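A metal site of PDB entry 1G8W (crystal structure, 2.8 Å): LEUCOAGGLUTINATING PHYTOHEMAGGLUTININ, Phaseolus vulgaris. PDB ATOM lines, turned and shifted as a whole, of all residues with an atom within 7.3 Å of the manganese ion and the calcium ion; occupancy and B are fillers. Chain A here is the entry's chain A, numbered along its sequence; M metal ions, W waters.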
ATOM      1  N   ASP A  86       5.554 -29.544  20.639  1.00  0.00           N
ATOM      2  CA  ASP A  86       5.029 -28.266  21.117  1.00  0.00           C
ATOM      3  C   ASP A  86       5.327 -28.074  22.604  1.00  0.00           C
ATOM      4  O   ASP A  86       5.418 -26.950  23.098  1.00  0.00           O
ATOM      5  CB  ASP A  86       3.520 -28.230  20.885  1.00  0.00           C
ATOM      6  CG  ASP A  86       3.122 -27.315  19.740  1.00  0.00           C
ATOM      7  OD1 ASP A  86       3.201 -26.075  19.907  1.00  0.00           O
ATOM      8  OD2 ASP A  86       2.736 -27.835  18.678  1.00  0.00           O
ATOM      9  N   GLY A  87       5.475 -29.187  23.333  1.00  0.00           N
ATOM     10  CA  GLY A  87       5.758 -29.101  24.753  1.00  0.00           C
ATOM     11  C   GLY A  87       5.260 -30.283  25.559  1.00  0.00           C
ATOM     12  O   GLY A  87       4.654 -31.227  25.031  1.00  0.00           O
ATOM     13  N   GLY A 103      -1.054 -29.838  19.201  1.00  0.00           N
ATOM     14  CA  GLY A 103      -0.115 -28.727  19.132  1.00  0.00           C
ATOM     15  C   GLY A 103       0.001 -27.804  20.333  1.00  0.00           C
ATOM     16  O   GLY A 103       0.103 -28.247  21.476  1.00  0.00           O
ATOM     17  N   GLY A 104      -0.018 -26.502  20.072  1.00  0.00           N
ATOM     18  CA  GLY A 104       0.111 -25.522  21.127  1.00  0.00           C
ATOM     19  C   GLY A 104      -0.812 -25.692  22.324  1.00  0.00           C
ATOM     20  O   GLY A 104      -0.549 -25.135  23.386  1.00  0.00           O
ATOM     21  N   PHE A 105      -1.892 -26.449  22.167  1.00  0.00           N
ATOM     22  CA  PHE A 105      -2.812 -26.650  23.275  1.00  0.00           C
ATOM     23  C   PHE A 105      -2.372 -27.764  24.229  1.00  0.00           C
ATOM     24  O   PHE A 105      -3.040 -28.027  25.237  1.00  0.00           O
ATOM     25  CB  PHE A 105      -4.206 -26.921  22.730  1.00  0.00           C
ATOM     26  CG  PHE A 105      -4.897 -25.689  22.259  1.00  0.00           C
ATOM     27  CD1 PHE A 105      -5.245 -24.692  23.166  1.00  0.00           C
ATOM     28  CD2 PHE A 105      -5.173 -25.493  20.912  1.00  0.00           C
ATOM     29  CE1 PHE A 105      -5.852 -23.516  22.728  1.00  0.00           C
ATOM     30  CE2 PHE A 105      -5.783 -24.326  20.471  1.00  0.00           C
ATOM     31  CZ  PHE A 105      -6.127 -23.342  21.382  1.00  0.00           C
ATOM     32  N   LEU A 106      -1.258 -28.402  23.906  1.00  0.00           N
ATOM     33  CA  LEU A 106      -0.697 -29.456  24.742  1.00  0.00           C
ATOM     34  C   LEU A 106      -1.660 -30.591  25.120  1.00  0.00           C
ATOM     35  O   LEU A 106      -1.390 -31.353  26.049  1.00  0.00           O
ATOM     36  CB  LEU A 106      -0.111 -28.823  25.991  1.00  0.00           C
ATOM     37  CG  LEU A 106       0.894 -27.704  25.701  1.00  0.00           C
ATOM     38  CD1 LEU A 106       1.357 -27.057  27.003  1.00  0.00           C
ATOM     39  CD2 LEU A 106       2.064 -28.285  24.951  1.00  0.00           C
ATOM     40  N   GLU A 122       3.296 -26.242  32.524  1.00  0.00           N
ATOM     41  CA  GLU A 122       3.793 -26.567  31.208  1.00  0.00           C
ATOM     42  C   GLU A 122       5.237 -26.246  30.963  1.00  0.00           C
ATOM     43  O   GLU A 122       5.822 -25.367  31.591  1.00  0.00           O
ATOM     44  CB  GLU A 122       2.976 -25.837  30.149  1.00  0.00           C
ATOM     45  CG  GLU A 122       3.024 -24.339  30.317  1.00  0.00           C
ATOM     46  CD  GLU A 122       2.419 -23.625  29.151  1.00  0.00           C
ATOM     47  OE1 GLU A 122       1.264 -23.937  28.800  1.00  0.00           O
ATOM     48  OE2 GLU A 122       3.094 -22.747  28.577  1.00  0.00           O
ATOM     49  N   PHE A 123       5.808 -26.990  30.025  1.00  0.00           N
ATOM     50  CA  PHE A 123       7.185 -26.802  29.590  1.00  0.00           C
ATOM     51  C   PHE A 123       7.076 -26.604  28.083  1.00  0.00           C
ATOM     52  O   PHE A 123       7.261 -27.515  27.287  1.00  0.00           O
ATOM     53  CB  PHE A 123       8.017 -28.022  29.971  1.00  0.00           C
ATOM     54  CG  PHE A 123       8.041 -28.271  31.444  1.00  0.00           C
ATOM     55  CD1 PHE A 123       7.025 -29.010  32.056  1.00  0.00           C
ATOM     56  CD2 PHE A 123       9.016 -27.681  32.249  1.00  0.00           C
ATOM     57  CE1 PHE A 123       6.975 -29.150  33.452  1.00  0.00           C
ATOM     58  CE2 PHE A 123       8.972 -27.802  33.650  1.00  0.00           C
ATOM     59  CZ  PHE A 123       7.955 -28.537  34.248  1.00  0.00           C
ATOM     60  N   ASP A 124       6.721 -25.360  27.744  1.00  0.00           N
ATOM     61  CA  ASP A 124       6.495 -24.875  26.389  1.00  0.00           C
ATOM     62  C   ASP A 124       7.756 -24.720  25.536  1.00  0.00           C
ATOM     63  O   ASP A 124       8.641 -23.936  25.855  1.00  0.00           O
ATOM     64  CB  ASP A 124       5.805 -23.524  26.474  1.00  0.00           C
ATOM     65  CG  ASP A 124       4.892 -23.283  25.331  1.00  0.00           C
ATOM     66  OD1 ASP A 124       5.226 -23.720  24.216  1.00  0.00           O
ATOM     67  OD2 ASP A 124       3.840 -22.650  25.562  1.00  0.00           O
ATOM     68  N   THR A 125       7.825 -25.445  24.430  1.00  0.00           N
ATOM     69  CA  THR A 125       9.003 -25.353  23.584  1.00  0.00           C
ATOM     70  C   THR A 125       8.792 -24.574  22.283  1.00  0.00           C
ATOM     71  O   THR A 125       9.759 -24.290  21.573  1.00  0.00           O
ATOM     72  CB  THR A 125       9.527 -26.761  23.224  1.00  0.00           C
ATOM     73  OG1 THR A 125       8.443 -27.555  22.733  1.00  0.00           O
ATOM     74  CG2 THR A 125      10.154 -27.422  24.448  1.00  0.00           C
ATOM     75  N   LEU A 126       7.546 -24.230  21.975  1.00  0.00           N
ATOM     76  CA  LEU A 126       7.235 -23.493  20.747  1.00  0.00           C
ATOM     77  C   LEU A 126       6.446 -22.225  21.010  1.00  0.00           C
ATOM     78  O   LEU A 126       5.486 -22.223  21.780  1.00  0.00           O
ATOM     79  CB  LEU A 126       6.464 -24.371  19.773  1.00  0.00           C
ATOM     80  CG  LEU A 126       6.226 -23.735  18.395  1.00  0.00           C
ATOM     81  CD1 LEU A 126       7.557 -23.384  17.736  1.00  0.00           C
ATOM     82  CD2 LEU A 126       5.435 -24.703  17.536  1.00  0.00           C
ATOM     83  N   TYR A 127       6.849 -21.147  20.333  1.00  0.00           N
ATOM     84  CA  TYR A 127       6.196 -19.850  20.490  1.00  0.00           C
ATOM     85  C   TYR A 127       4.860 -19.727  19.747  1.00  0.00           C
ATOM     86  O   TYR A 127       4.797 -19.961  18.542  1.00  0.00           O
ATOM     87  CB  TYR A 127       7.148 -18.737  20.009  1.00  0.00           C
ATOM     88  CG  TYR A 127       6.534 -17.356  19.975  1.00  0.00           C
ATOM     89  CD1 TYR A 127       6.072 -16.740  21.138  1.00  0.00           C
ATOM     90  CD2 TYR A 127       6.368 -16.690  18.765  1.00  0.00           C
ATOM     91  CE1 TYR A 127       5.456 -15.498  21.101  1.00  0.00           C
ATOM     92  CE2 TYR A 127       5.755 -15.435  18.718  1.00  0.00           C
ATOM     93  CZ  TYR A 127       5.294 -14.846  19.895  1.00  0.00           C
ATOM     94  OH  TYR A 127       4.662 -13.632  19.858  1.00  0.00           O
ATOM     95  N   ASN A 128       3.799 -19.374  20.458  1.00  0.00           N
ATOM     96  CA  ASN A 128       2.482 -19.187  19.850  1.00  0.00           C
ATOM     97  C   ASN A 128       2.087 -17.724  19.979  1.00  0.00           C
ATOM     98  O   ASN A 128       1.692 -17.278  21.054  1.00  0.00           O
ATOM     99  CB  ASN A 128       1.413 -20.041  20.548  1.00  0.00           C
ATOM    100  CG  ASN A 128       1.696 -21.522  20.455  1.00  0.00           C
ATOM    101  OD1 ASN A 128       2.433 -22.074  21.272  1.00  0.00           O
ATOM    102  ND2 ASN A 128       1.126 -22.175  19.457  1.00  0.00           N
ATOM    103  N   TRP A 131      -0.740 -16.129  22.554  1.00  0.00           N
ATOM    104  CA  TRP A 131      -0.752 -16.139  24.023  1.00  0.00           C
ATOM    105  C   TRP A 131       0.575 -16.408  24.717  1.00  0.00           C
ATOM    106  O   TRP A 131       0.691 -16.166  25.915  1.00  0.00           O
ATOM    107  CB  TRP A 131      -1.763 -17.197  24.492  1.00  0.00           C
ATOM    108  CG  TRP A 131      -1.412 -18.597  24.022  1.00  0.00           C
ATOM    109  CD1 TRP A 131      -0.322 -19.345  24.404  1.00  0.00           C
ATOM    110  CD2 TRP A 131      -2.092 -19.380  23.035  1.00  0.00           C
ATOM    111  NE1 TRP A 131      -0.297 -20.529  23.719  1.00  0.00           N
ATOM    112  CE2 TRP A 131      -1.362 -20.580  22.866  1.00  0.00           C
ATOM    113  CE3 TRP A 131      -3.256 -19.186  22.269  1.00  0.00           C
ATOM    114  CZ2 TRP A 131      -1.754 -21.586  21.967  1.00  0.00           C
ATOM    115  CZ3 TRP A 131      -3.645 -20.183  21.373  1.00  0.00           C
ATOM    116  CH2 TRP A 131      -2.892 -21.367  21.238  1.00  0.00           C
ATOM    117  N   ASP A 132       1.561 -16.917  23.994  1.00  0.00           N
ATOM    118  CA  ASP A 132       2.852 -17.246  24.591  1.00  0.00           C
ATOM    119  C   ASP A 132       3.850 -16.112  24.652  1.00  0.00           C
ATOM    120  O   ASP A 132       3.825 -15.207  23.830  1.00  0.00           O
ATOM    121  CB  ASP A 132       3.545 -18.388  23.823  1.00  0.00           C
ATOM    122  CG  ASP A 132       3.155 -19.765  24.312  1.00  0.00           C
ATOM    123  OD1 ASP A 132       2.795 -19.923  25.493  1.00  0.00           O
ATOM    124  OD2 ASP A 132       3.232 -20.715  23.501  1.00  0.00           O
ATOM    125  N   PRO A 133       4.741 -16.136  25.659  1.00  0.00           N
ATOM    126  CA  PRO A 133       5.762 -15.101  25.780  1.00  0.00           C
ATOM    127  C   PRO A 133       6.749 -15.409  24.635  1.00  0.00           C
ATOM    128  O   PRO A 133       6.687 -16.496  24.048  1.00  0.00           O
ATOM    129  CB  PRO A 133       6.349 -15.341  27.170  1.00  0.00           C
ATOM    130  CG  PRO A 133       6.074 -16.766  27.428  1.00  0.00           C
ATOM    131  CD  PRO A 133       4.685 -16.943  26.888  1.00  0.00           C
ATOM    132  N   GLU A 135      10.056 -16.151  24.487  1.00  0.00           N
ATOM    133  CA  GLU A 135      11.019 -17.230  24.639  1.00  0.00           C
ATOM    134  C   GLU A 135      10.408 -18.493  25.241  1.00  0.00           C
ATOM    135  O   GLU A 135       9.335 -18.451  25.835  1.00  0.00           O
ATOM    136  CB  GLU A 135      12.185 -16.766  25.489  1.00  0.00           C
ATOM    137  CG  GLU A 135      12.833 -15.487  24.985  1.00  0.00           C
ATOM    138  CD  GLU A 135      14.173 -15.215  25.627  1.00  0.00           C
ATOM    139  OE1 GLU A 135      15.156 -15.915  25.284  1.00  0.00           O
ATOM    140  OE2 GLU A 135      14.250 -14.317  26.491  1.00  0.00           O
ATOM    141  N   HIS A 137       9.514 -21.301  27.731  1.00  0.00           N
ATOM    142  CA  HIS A 137       9.267 -21.070  29.144  1.00  0.00           C
ATOM    143  C   HIS A 137       8.623 -22.211  29.930  1.00  0.00           C
ATOM    144  O   HIS A 137       8.222 -23.238  29.393  1.00  0.00           O
ATOM    145  CB  HIS A 137       8.332 -19.881  29.228  1.00  0.00           C
ATOM    146  CG  HIS A 137       7.172 -19.999  28.293  1.00  0.00           C
ATOM    147  ND1 HIS A 137       7.302 -19.849  26.926  1.00  0.00           N
ATOM    148  CD2 HIS A 137       5.881 -20.367  28.497  1.00  0.00           C
ATOM    149  CE1 HIS A 137       6.158 -20.131  26.333  1.00  0.00           C
ATOM    150  NE2 HIS A 137       5.278 -20.458  27.263  1.00  0.00           N
ATOM    151  N   ILE A 138       8.524 -21.964  31.232  1.00  0.00           N
ATOM    152  CA  ILE A 138       7.862 -22.857  32.163  1.00  0.00           C
ATOM    153  C   ILE A 138       6.677 -21.982  32.571  1.00  0.00           C
ATOM    154  O   ILE A 138       6.858 -20.802  32.879  1.00  0.00           O
ATOM    155  CB  ILE A 138       8.714 -23.116  33.399  1.00  0.00           C
ATOM    156  CG1 ILE A 138      10.007 -23.819  32.992  1.00  0.00           C
ATOM    157  CG2 ILE A 138       7.959 -23.994  34.381  1.00  0.00           C
ATOM    158  CD1 ILE A 138      10.987 -24.007  34.141  1.00  0.00           C
ATOM    159  N   GLY A 139       5.461 -22.535  32.536  1.00  0.00           N
ATOM    160  CA  GLY A 139       4.309 -21.736  32.906  1.00  0.00           C
ATOM    161  C   GLY A 139       3.282 -22.448  33.746  1.00  0.00           C
ATOM    162  O   GLY A 139       3.110 -23.673  33.631  1.00  0.00           O
ATOM    163  N   ASP A 141      -0.460 -22.964  34.279  1.00  0.00           N
ATOM    164  CA  ASP A 141      -1.730 -22.805  33.566  1.00  0.00           C
ATOM    165  C   ASP A 141      -2.949 -23.127  34.429  1.00  0.00           C
ATOM    166  O   ASP A 141      -3.075 -24.237  34.948  1.00  0.00           O
ATOM    167  CB  ASP A 141      -1.780 -23.721  32.343  1.00  0.00           C
ATOM    168  CG  ASP A 141      -0.632 -23.483  31.393  1.00  0.00           C
ATOM    169  OD1 ASP A 141       0.121 -22.522  31.612  1.00  0.00           O
ATOM    170  OD2 ASP A 141      -0.494 -24.260  30.439  1.00  0.00           O
ATOM    171  N   ILE A 145      -4.627 -22.073  28.151  1.00  0.00           N
ATOM    172  CA  ILE A 145      -3.313 -22.351  27.593  1.00  0.00           C
ATOM    173  C   ILE A 145      -2.443 -21.097  27.795  1.00  0.00           C
ATOM    174  O   ILE A 145      -1.228 -21.153  27.642  1.00  0.00           O
ATOM    175  CB  ILE A 145      -3.418 -22.721  26.100  1.00  0.00           C
ATOM    176  CG1 ILE A 145      -2.094 -23.336  25.615  1.00  0.00           C
ATOM    177  CG2 ILE A 145      -3.751 -21.492  25.278  1.00  0.00           C
ATOM    178  CD1 ILE A 145      -1.740 -24.637  26.284  1.00  0.00           C
ATOM    179  N   ARG A 146      -3.072 -19.974  28.130  1.00  0.00           N
ATOM    180  CA  ARG A 146      -2.368 -18.727  28.387  1.00  0.00           C
ATOM    181  C   ARG A 146      -1.963 -18.727  29.860  1.00  0.00           C
ATOM    182  O   ARG A 146      -2.768 -18.421  30.725  1.00  0.00           O
ATOM    183  CB  ARG A 146      -3.270 -17.520  28.130  1.00  0.00           C
ATOM    184  N   SER A 147      -0.711 -19.063  30.133  1.00  0.00           N
ATOM    185  CA  SER A 147      -0.200 -19.142  31.498  1.00  0.00           C
ATOM    186  C   SER A 147      -0.459 -17.905  32.338  1.00  0.00           C
ATOM    187  O   SER A 147      -0.306 -16.777  31.881  1.00  0.00           O
ATOM    188  CB  SER A 147       1.289 -19.441  31.487  1.00  0.00           C
ATOM    189  OG  SER A 147       1.557 -20.589  30.709  1.00  0.00           O
ATOM    190  N   THR A 150       4.816 -16.983  33.949  1.00  0.00           N
ATOM    191  CA  THR A 150       5.860 -17.820  33.366  1.00  0.00           C
ATOM    192  C   THR A 150       7.266 -17.397  33.777  1.00  0.00           C
ATOM    193  O   THR A 150       7.450 -16.456  34.561  1.00  0.00           O
ATOM    194  CB  THR A 150       5.818 -17.781  31.811  1.00  0.00           C
ATOM    195  OG1 THR A 150       6.226 -16.486  31.365  1.00  0.00           O
ATOM    196  CG2 THR A 150       4.429 -18.073  31.298  1.00  0.00           C
HETATM  197 MN    MN M   1       3.196 -21.330  27.285  1.00  0.00          MN
HETATM  198 CA    CA M   2       3.586 -23.045  22.950  1.00  0.00          CA
HETATM  199  O   HOH W   1       1.565 -23.657  23.963  1.00  0.00           O
HETATM  200  O   HOH W   2       2.098 -19.801  28.207  1.00  0.00           O
HETATM  201  O   HOH W   3       1.366 -22.332  26.466  1.00  0.00           O
HETATM  202  O   HOH W   4       3.164 -25.240  22.191  1.00  0.00           O
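Residues that only touch the manganese ion: Ser 147 (3.9 Å).
Of the 25 residues printed, 5 come within 4 Å of the manganese ion.
ND1 of His 137 lies within hydrogen-bond range of O of Glu 135 (2.7 Å).
OE1 of Glu 122 sits close to OD2 of Asp 141, 2.4 Å away.
The side-chain carboxylate of Asp 141 is in hydrogen-bond range of the side-chain hydroxyl of Ser 147 (2.6 Å).
N of Glu 122 is in hydrogen-bond range of O of Gly 139.
OE2 of Glu 122 sits close to OG of Ser 147 (3.4 Å).
Within 4 Å of the calcium ion: Asp 124, Leu 126, Asn 128 and Asp 132.
The nearest printed residue that does not touch the calcium ion is Asp 86 (4.3 Å).
The side-chain carboxylate (OE2) of Glu 122 binds the manganese ion (1.9 Å).
Water W2 binds the manganese ion (2.1 Å).
Water W3 binds the manganese ion.
NE2 of His 137 is bound to the manganese ion (2.3 Å).
The side-chain carboxylate (OD2) of Asp 124 binds the manganese ion.
OD1 of Asp 132 binds the manganese ion (2.3 Å).
Water W3 lies within hydrogen-bond range of OE1 of Glu 122 and O of Ile 145.
The calcium ion is bound by OD1 of Asp 124 (2.2 Å), OD1 of Asn 128 (2.3 Å), water W1 (2.3 Å), water W4 (2.4 Å), O of Leu 126 (2.4 Å), OD2 of Asp 132 (2.4 Å) and OD2 of Asp 124 (2.7 Å).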
